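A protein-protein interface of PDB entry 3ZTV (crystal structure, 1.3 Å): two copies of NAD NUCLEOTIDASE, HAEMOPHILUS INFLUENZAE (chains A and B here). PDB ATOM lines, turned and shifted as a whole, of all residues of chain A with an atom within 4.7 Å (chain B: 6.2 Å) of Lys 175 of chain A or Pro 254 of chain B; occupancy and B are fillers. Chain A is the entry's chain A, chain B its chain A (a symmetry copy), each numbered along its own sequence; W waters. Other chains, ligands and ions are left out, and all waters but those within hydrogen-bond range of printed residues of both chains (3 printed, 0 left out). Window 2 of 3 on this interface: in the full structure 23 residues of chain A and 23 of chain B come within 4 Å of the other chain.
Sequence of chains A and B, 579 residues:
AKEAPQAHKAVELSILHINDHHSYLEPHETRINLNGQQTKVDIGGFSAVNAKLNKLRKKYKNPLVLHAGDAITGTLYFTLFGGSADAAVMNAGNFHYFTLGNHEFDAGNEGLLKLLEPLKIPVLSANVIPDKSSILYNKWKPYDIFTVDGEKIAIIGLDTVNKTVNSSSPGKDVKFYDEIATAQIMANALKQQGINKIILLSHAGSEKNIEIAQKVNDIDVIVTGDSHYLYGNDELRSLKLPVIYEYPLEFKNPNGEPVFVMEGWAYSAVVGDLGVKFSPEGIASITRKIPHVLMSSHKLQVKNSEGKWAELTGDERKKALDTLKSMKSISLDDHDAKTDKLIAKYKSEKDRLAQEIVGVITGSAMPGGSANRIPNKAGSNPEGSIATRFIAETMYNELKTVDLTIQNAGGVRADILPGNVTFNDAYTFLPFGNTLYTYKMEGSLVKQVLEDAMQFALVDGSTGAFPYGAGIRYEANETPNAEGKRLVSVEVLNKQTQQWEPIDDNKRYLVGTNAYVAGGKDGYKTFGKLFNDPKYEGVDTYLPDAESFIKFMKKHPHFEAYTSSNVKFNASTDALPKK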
ATOM      1  N   ASN A 127      -8.679 -15.602 -29.613  1.00  0.00           N
ATOM      2  CA  ASN A 127      -8.810 -17.026 -29.300  1.00  0.00           C
ATOM      3  C   ASN A 127      -7.459 -17.691 -29.001  1.00  0.00           C
ATOM      4  O   ASN A 127      -7.371 -18.924 -28.923  1.00  0.00           O
ATOM      5  CB  ASN A 127      -9.576 -17.792 -30.393  1.00  0.00           C
ATOM      6  CG  ASN A 127      -8.815 -17.873 -31.708  1.00  0.00           C
ATOM      7  OD1 ASN A 127      -8.093 -16.951 -32.085  1.00  0.00           O
ATOM      8  ND2 ASN A 127      -9.001 -18.973 -32.419  1.00  0.00           N
ATOM      9  N   VAL A 128      -6.411 -16.877 -28.843  1.00  0.00           N
ATOM     10  CA  VAL A 128      -5.082 -17.356 -28.475  1.00  0.00           C
ATOM     11  C   VAL A 128      -4.706 -16.573 -27.222  1.00  0.00           C
ATOM     12  O   VAL A 128      -4.491 -15.357 -27.278  1.00  0.00           O
ATOM     13  CB  VAL A 128      -4.069 -17.114 -29.608  1.00  0.00           C
ATOM     14  CG1 VAL A 128      -2.721 -17.718 -29.239  1.00  0.00           C
ATOM     15  CG2 VAL A 128      -4.591 -17.694 -30.926  1.00  0.00           C
ATOM     16  N   ILE A 129      -4.657 -17.253 -26.078  1.00  0.00           N
ATOM     17  CA  ILE A 129      -4.607 -16.559 -24.791  1.00  0.00           C
ATOM     18  C   ILE A 129      -3.499 -17.134 -23.891  1.00  0.00           C
ATOM     19  O   ILE A 129      -3.611 -18.261 -23.410  1.00  0.00           O
ATOM     20  CB  ILE A 129      -5.984 -16.618 -24.048  1.00  0.00           C
ATOM     21  CG1 ILE A 129      -7.125 -16.162 -24.967  1.00  0.00           C
ATOM     22  CG2 ILE A 129      -5.953 -15.730 -22.819  1.00  0.00           C
ATOM     23  CD1 ILE A 129      -8.521 -16.242 -24.304  1.00  0.00           C
ATOM     24  N   ASP A 131      -1.225 -17.837 -20.605  1.00  0.00           N
ATOM     25  CA  ASP A 131      -1.291 -17.824 -19.150  1.00  0.00           C
ATOM     26  C   ASP A 131      -0.303 -16.800 -18.597  1.00  0.00           C
ATOM     27  O   ASP A 131       0.628 -16.373 -19.293  1.00  0.00           O
ATOM     28  CB  ASP A 131      -0.979 -19.214 -18.578  1.00  0.00           C
ATOM     29  CG  ASP A 131      -2.055 -20.242 -18.886  1.00  0.00           C
ATOM     30  OD1 ASP A 131      -3.220 -19.868 -19.077  1.00  0.00           O
ATOM     31  OD2 ASP A 131      -1.731 -21.448 -18.898  1.00  0.00           O
ATOM     32  N   LYS A 172       3.028 -24.666 -24.217  1.00  0.00           N
ATOM     33  CA  LYS A 172       1.876 -25.218 -23.507  1.00  0.00           C
ATOM     34  C   LYS A 172       1.121 -24.168 -22.692  1.00  0.00           C
ATOM     35  O   LYS A 172      -0.037 -24.375 -22.326  1.00  0.00           O
ATOM     36  CB  LYS A 172       2.303 -26.384 -22.603  1.00  0.00           C
ATOM     37  CG  LYS A 172       2.960 -25.974 -21.281  1.00  0.00           C
ATOM     38  CD  LYS A 172       4.239 -25.185 -21.499  1.00  0.00           C
ATOM     39  CE  LYS A 172       5.072 -25.066 -20.224  1.00  0.00           C
ATOM     40  NZ  LYS A 172       4.422 -24.255 -19.150  1.00  0.00           N
ATOM     41  N   ASP A 173       1.772 -23.047 -22.399  1.00  0.00           N
ATOM     42  CA  ASP A 173       1.143 -21.988 -21.616  1.00  0.00           C
ATOM     43  C   ASP A 173       0.309 -21.034 -22.472  1.00  0.00           C
ATOM     44  O   ASP A 173      -0.164 -20.008 -21.979  1.00  0.00           O
ATOM     45  CB  ASP A 173       2.164 -21.219 -20.764  1.00  0.00           C
ATOM     46  CG  ASP A 173       3.283 -20.599 -21.585  1.00  0.00           C
ATOM     47  OD1 ASP A 173       3.051 -20.205 -22.748  1.00  0.00           O
ATOM     48  OD2 ASP A 173       4.412 -20.490 -21.047  1.00  0.00           O
ATOM     49  N   VAL A 174       0.158 -21.370 -23.749  1.00  0.00           N
ATOM     50  CA  VAL A 174      -0.734 -20.630 -24.647  1.00  0.00           C
ATOM     51  C   VAL A 174      -1.971 -21.472 -24.929  1.00  0.00           C
ATOM     52  O   VAL A 174      -1.863 -22.577 -25.443  1.00  0.00           O
ATOM     53  CB  VAL A 174      -0.039 -20.296 -25.973  1.00  0.00           C
ATOM     54  CG1 VAL A 174      -0.991 -19.506 -26.874  1.00  0.00           C
ATOM     55  CG2 VAL A 174       1.227 -19.502 -25.701  1.00  0.00           C
ATOM     56  N   LYS A 175      -3.145 -20.946 -24.582  1.00  0.00           N
ATOM     57  CA  LYS A 175      -4.397 -21.677 -24.747  1.00  0.00           C
ATOM     58  C   LYS A 175      -5.169 -21.195 -25.977  1.00  0.00           C
ATOM     59  O   LYS A 175      -5.244 -19.992 -26.251  1.00  0.00           O
ATOM     60  CB  LYS A 175      -5.251 -21.548 -23.478  1.00  0.00           C
ATOM     61  CG  LYS A 175      -4.955 -22.588 -22.378  1.00  0.00           C
ATOM     62  CD  LYS A 175      -3.494 -22.629 -21.968  1.00  0.00           C
ATOM     63  CE  LYS A 175      -3.268 -23.590 -20.795  1.00  0.00           C
ATOM     64  NZ  LYS A 175      -3.824 -23.078 -19.496  1.00  0.00           N
ATOM     65  N   PHE A 176      -5.729 -22.149 -26.713  1.00  0.00           N
ATOM     66  CA  PHE A 176      -6.474 -21.859 -27.942  1.00  0.00           C
ATOM     67  C   PHE A 176      -7.954 -22.184 -27.771  1.00  0.00           C
ATOM     68  O   PHE A 176      -8.306 -23.166 -27.118  1.00  0.00           O
ATOM     69  CB  PHE A 176      -5.929 -22.699 -29.101  1.00  0.00           C
ATOM     70  CG  PHE A 176      -4.563 -22.276 -29.581  1.00  0.00           C
ATOM     71  CD1 PHE A 176      -3.415 -22.599 -28.861  1.00  0.00           C
ATOM     72  CD2 PHE A 176      -4.423 -21.558 -30.765  1.00  0.00           C
ATOM     73  CE1 PHE A 176      -2.158 -22.204 -29.315  1.00  0.00           C
ATOM     74  CE2 PHE A 176      -3.167 -21.163 -31.216  1.00  0.00           C
ATOM     75  CZ  PHE A 176      -2.038 -21.489 -30.486  1.00  0.00           C
ATOM     76  N   TYR A 177      -8.813 -21.377 -28.389  1.00  0.00           N
ATOM     77  CA  TYR A 177     -10.265 -21.545 -28.321  1.00  0.00           C
ATOM     78  C   TYR A 177     -10.900 -21.572 -29.712  1.00  0.00           C
ATOM     79  O   TYR A 177     -10.413 -20.939 -30.660  1.00  0.00           O
ATOM     80  CB  TYR A 177     -10.867 -20.462 -27.414  1.00  0.00           C
ATOM     81  CG  TYR A 177     -10.367 -20.653 -26.000  1.00  0.00           C
ATOM     82  CD1 TYR A 177     -11.011 -21.525 -25.129  1.00  0.00           C
ATOM     83  CD2 TYR A 177      -9.201 -20.032 -25.557  1.00  0.00           C
ATOM     84  CE1 TYR A 177     -10.532 -21.742 -23.843  1.00  0.00           C
ATOM     85  CE2 TYR A 177      -8.716 -20.242 -24.276  1.00  0.00           C
ATOM     86  CZ  TYR A 177      -9.380 -21.098 -23.426  1.00  0.00           C
ATOM     87  OH  TYR A 177      -8.876 -21.319 -22.156  1.00  0.00           O
ATOM     88  N   ILE B 212     -14.382 -25.336 -14.758  1.00  0.00           N
ATOM     89  CA  ILE B 212     -14.105 -23.960 -15.133  1.00  0.00           C
ATOM     90  C   ILE B 212     -13.116 -23.308 -14.155  1.00  0.00           C
ATOM     91  O   ILE B 212     -12.152 -22.640 -14.576  1.00  0.00           O
ATOM     92  CB  ILE B 212     -15.416 -23.141 -15.242  1.00  0.00           C
ATOM     93  CG1 ILE B 212     -16.246 -23.616 -16.441  1.00  0.00           C
ATOM     94  CG2 ILE B 212     -15.131 -21.655 -15.339  1.00  0.00           C
ATOM     95  CD1 ILE B 212     -17.660 -23.024 -16.509  1.00  0.00           C
ATOM     96  N   ALA B 213     -13.340 -23.518 -12.858  1.00  0.00           N
ATOM     97  CA  ALA B 213     -12.459 -22.945 -11.839  1.00  0.00           C
ATOM     98  C   ALA B 213     -11.004 -23.355 -12.054  1.00  0.00           C
ATOM     99  O   ALA B 213     -10.091 -22.560 -11.839  1.00  0.00           O
ATOM    100  CB  ALA B 213     -12.919 -23.345 -10.451  1.00  0.00           C
ATOM    101  N   GLN B 214     -10.792 -24.589 -12.511  1.00  0.00           N
ATOM    102  CA  GLN B 214      -9.435 -25.125 -12.649  1.00  0.00           C
ATOM    103  C   GLN B 214      -8.818 -24.900 -14.022  1.00  0.00           C
ATOM    104  O   GLN B 214      -7.596 -25.008 -14.176  1.00  0.00           O
ATOM    105  CB  GLN B 214      -9.426 -26.610 -12.312  1.00  0.00           C
ATOM    106  CG  GLN B 214      -9.768 -26.890 -10.860  1.00  0.00           C
ATOM    107  CD  GLN B 214      -9.895 -28.366 -10.576  1.00  0.00           C
ATOM    108  OE1 GLN B 214     -10.932 -28.970 -10.847  1.00  0.00           O
ATOM    109  NE2 GLN B 214      -8.841 -28.961 -10.033  1.00  0.00           N
ATOM    110  N   LYS B 215      -9.646 -24.573 -15.010  1.00  0.00           N
ATOM    111  CA  LYS B 215      -9.188 -24.480 -16.399  1.00  0.00           C
ATOM    112  C   LYS B 215      -9.267 -23.090 -17.006  1.00  0.00           C
ATOM    113  O   LYS B 215      -8.717 -22.852 -18.078  1.00  0.00           O
ATOM    114  CB  LYS B 215      -9.960 -25.460 -17.287  1.00  0.00           C
ATOM    115  CG  LYS B 215      -9.672 -26.917 -16.988  1.00  0.00           C
ATOM    116  CD  LYS B 215     -10.330 -27.852 -17.989  1.00  0.00           C
ATOM    117  CE  LYS B 215      -9.932 -29.297 -17.721  1.00  0.00           C
ATOM    118  NZ  LYS B 215     -10.621 -30.249 -18.640  1.00  0.00           N
ATOM    119  N   VAL B 216      -9.956 -22.172 -16.340  1.00  0.00           N
ATOM    120  CA  VAL B 216     -10.226 -20.851 -16.888  1.00  0.00           C
ATOM    121  C   VAL B 216      -9.665 -19.784 -15.950  1.00  0.00           C
ATOM    122  O   VAL B 216      -9.826 -19.883 -14.732  1.00  0.00           O
ATOM    123  CB  VAL B 216     -11.756 -20.643 -17.079  1.00  0.00           C
ATOM    124  CG1 VAL B 216     -12.087 -19.206 -17.440  1.00  0.00           C
ATOM    125  CG2 VAL B 216     -12.309 -21.614 -18.126  1.00  0.00           C
ATOM    126  N   ASN B 217      -9.006 -18.782 -16.526  1.00  0.00           N
ATOM    127  CA  ASN B 217      -8.445 -17.674 -15.755  1.00  0.00           C
ATOM    128  C   ASN B 217      -9.390 -16.481 -15.601  1.00  0.00           C
ATOM    129  O   ASN B 217     -10.349 -16.314 -16.365  1.00  0.00           O
ATOM    130  CB  ASN B 217      -7.126 -17.186 -16.386  1.00  0.00           C
ATOM    131  CG  ASN B 217      -6.056 -18.256 -16.410  1.00  0.00           C
ATOM    132  OD1 ASN B 217      -5.405 -18.493 -17.442  1.00  0.00           O
ATOM    133  ND2 ASN B 217      -5.874 -18.916 -15.285  1.00  0.00           N
ATOM    134  N   LYS B 252      -7.355 -23.325  -7.392  1.00  0.00           N
ATOM    135  CA  LYS B 252      -6.477 -22.402  -8.104  1.00  0.00           C
ATOM    136  C   LYS B 252      -6.734 -22.518  -9.602  1.00  0.00           C
ATOM    137  O   LYS B 252      -6.850 -23.629 -10.134  1.00  0.00           O
ATOM    138  CB  LYS B 252      -5.000 -22.728  -7.845  1.00  0.00           C
ATOM    139  CG  LYS B 252      -4.407 -22.163  -6.561  1.00  0.00           C
ATOM    140  CD  LYS B 252      -2.904 -22.477  -6.480  1.00  0.00           C
ATOM    141  CE  LYS B 252      -2.265 -21.942  -5.205  1.00  0.00           C
ATOM    142  NZ  LYS B 252      -2.194 -20.458  -5.189  1.00  0.00           N
ATOM    143  N   ASN B 253      -6.811 -21.386 -10.282  1.00  0.00           N
ATOM    144  CA  ASN B 253      -6.899 -21.414 -11.730  1.00  0.00           C
ATOM    145  C   ASN B 253      -5.495 -21.612 -12.329  1.00  0.00           C
ATOM    146  O   ASN B 253      -4.505 -21.670 -11.582  1.00  0.00           O
ATOM    147  CB  ASN B 253      -7.639 -20.173 -12.257  1.00  0.00           C
ATOM    148  CG  ASN B 253      -6.877 -18.867 -12.039  1.00  0.00           C
ATOM    149  OD1 ASN B 253      -5.662 -18.865 -11.804  1.00  0.00           O
ATOM    150  ND2 ASN B 253      -7.591 -17.748 -12.132  1.00  0.00           N
ATOM    151  N   PRO B 254      -5.384 -21.750 -13.663  1.00  0.00           N
ATOM    152  CA  PRO B 254      -4.062 -22.012 -14.250  1.00  0.00           C
ATOM    153  C   PRO B 254      -3.037 -20.930 -13.911  1.00  0.00           C
ATOM    154  O   PRO B 254      -1.831 -21.226 -13.845  1.00  0.00           O
ATOM    155  CB  PRO B 254      -4.359 -22.063 -15.751  1.00  0.00           C
ATOM    156  CG  PRO B 254      -5.789 -22.603 -15.804  1.00  0.00           C
ATOM    157  CD  PRO B 254      -6.476 -21.929 -14.638  1.00  0.00           C
ATOM    158  N   ASN B 255      -3.495 -19.706 -13.679  1.00  0.00           N
ATOM    159  CA  ASN B 255      -2.617 -18.597 -13.324  1.00  0.00           C
ATOM    160  C   ASN B 255      -2.196 -18.605 -11.858  1.00  0.00           C
ATOM    161  O   ASN B 255      -1.328 -17.818 -11.457  1.00  0.00           O
ATOM    162  CB  ASN B 255      -3.258 -17.258 -13.692  1.00  0.00           C
ATOM    163  CG  ASN B 255      -3.227 -17.003 -15.183  1.00  0.00           C
ATOM    164  OD1 ASN B 255      -2.588 -17.748 -15.924  1.00  0.00           O
ATOM    165  ND2 ASN B 255      -3.913 -15.957 -15.632  1.00  0.00           N
ATOM    166  N   GLY B 256      -2.796 -19.489 -11.064  1.00  0.00           N
ATOM    167  CA  GLY B 256      -2.450 -19.618  -9.661  1.00  0.00           C
ATOM    168  C   GLY B 256      -3.326 -18.801  -8.729  1.00  0.00           C
ATOM    169  O   GLY B 256      -3.098 -18.807  -7.526  1.00  0.00           O
ATOM    170  N   GLU B 257      -4.340 -18.113  -9.264  1.00  0.00           N
ATOM    171  CA  GLU B 257      -5.230 -17.291  -8.434  1.00  0.00           C
ATOM    172  C   GLU B 257      -6.367 -18.124  -7.834  1.00  0.00           C
ATOM    173  O   GLU B 257      -6.791 -19.109  -8.427  1.00  0.00           O
ATOM    174  CB  GLU B 257      -5.788 -16.122  -9.254  1.00  0.00           C
ATOM    175  CG  GLU B 257      -4.693 -15.312  -9.973  1.00  0.00           C
ATOM    176  CD  GLU B 257      -3.613 -14.798  -9.053  1.00  0.00           C
ATOM    177  OE1 GLU B 257      -3.115 -15.561  -8.196  1.00  0.00           O
ATOM    178  OE2 GLU B 257      -3.239 -13.613  -9.195  1.00  0.00           O
HETATM  179  O   HOH W   1      -6.734 -24.447 -19.206  1.00  0.00           O
HETATM  180  O   HOH W   2      -6.363 -21.977 -19.290  1.00  0.00           O
HETATM  181  O   HOH W   3     -10.001 -23.320 -20.598  1.00  0.00           O
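No position is printed for both chains.
Of the 3 pairs that touch across the chains among the printed residues, none has its exchanged pair printed and touching as well.
Of the 10 printed residues of chain A, 2 touch a printed residue of chain B.
Printed residues of chain B that touch a printed residue of chain A: Asn 217, Pro 254 and Asn 255.
Hydrophobic or aromatic side chains of chain B within 4 Å of the printed part of chain A: Pro 254.
Among the printed residues, 3 pairs touch across the chains.
Among the printed residues, merely in contact across the chains: Asp 131 of chain A with Asn 255 of chain B and Lys 175 of chain A with Pro 254 of chain B.
The backbone carbonyl oxygen (O) of Lys 175 of chain A lies within hydrogen-bond range of the backbone NH (N) of Ile 129 of chain A, at 2.8 Å.
The side-chain amide oxygen of Asn 253 of chain B lies close to the side-chain amide nitrogen of Asn 217 of chain B, 3.5 Å away.
O of Asp 173 of chain A lies within hydrogen-bond range of N of Asp 131 of chain A, at 2.8 Å.
OD1 of Asn 253 of chain B lies within hydrogen-bond range of N of Asn 255 of chain B (3.0 Å).
The side-chain carboxylate of Asp 131 of chain A lies within salt-bridge range of the side-chain amino group of Lys 175 of chain A.
N of Asn 255 of chain B sits close to ND2 of Asn 217 of chain B (3.0 Å).
Of the printed residues of chain B, Asp 131 of chain A touches Asn 217 (3.1 Å) and Asn 255 (3.4 Å).
Printed residues of chain B within 4 Å of Lys 175 of chain A: Pro 254.
Ala 213 of chain B touches none of the printed residues of chain A.
Of the printed residues of chain A, Asn 217 of chain B touches Asp 131 (3.1 Å).
Printed residues of chain A within 4 Å of Asn 255 of chain B: Asp 131.
The nearest residue of chain B that does not touch Lys 175 of chain A is Lys 215 of chain B (5.1 Å).
The nearest residue of chain A that does not touch Pro 254 of chain B is Asp 131 of chain A (4.1 Å).
Water W3 bridges the side-chain hydroxyl of Tyr 177 of chain A (2.8 Å) and the backbone carbonyl oxygen of Lys 215 of chain B (2.9 Å).
Water W2 lies within hydrogen-bond range of NZ of Lys 175 of chain A and O of Lys 215 of chain B.
Water W1 lies within hydrogen-bond range of O of Lys 215 of chain B and NZ of Lys 175 of chain A.
The side-chain carboxylate of Asp 131 of chain A lies close to the side-chain amide oxygen of Asn 217 of chain B (3.1 Å).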
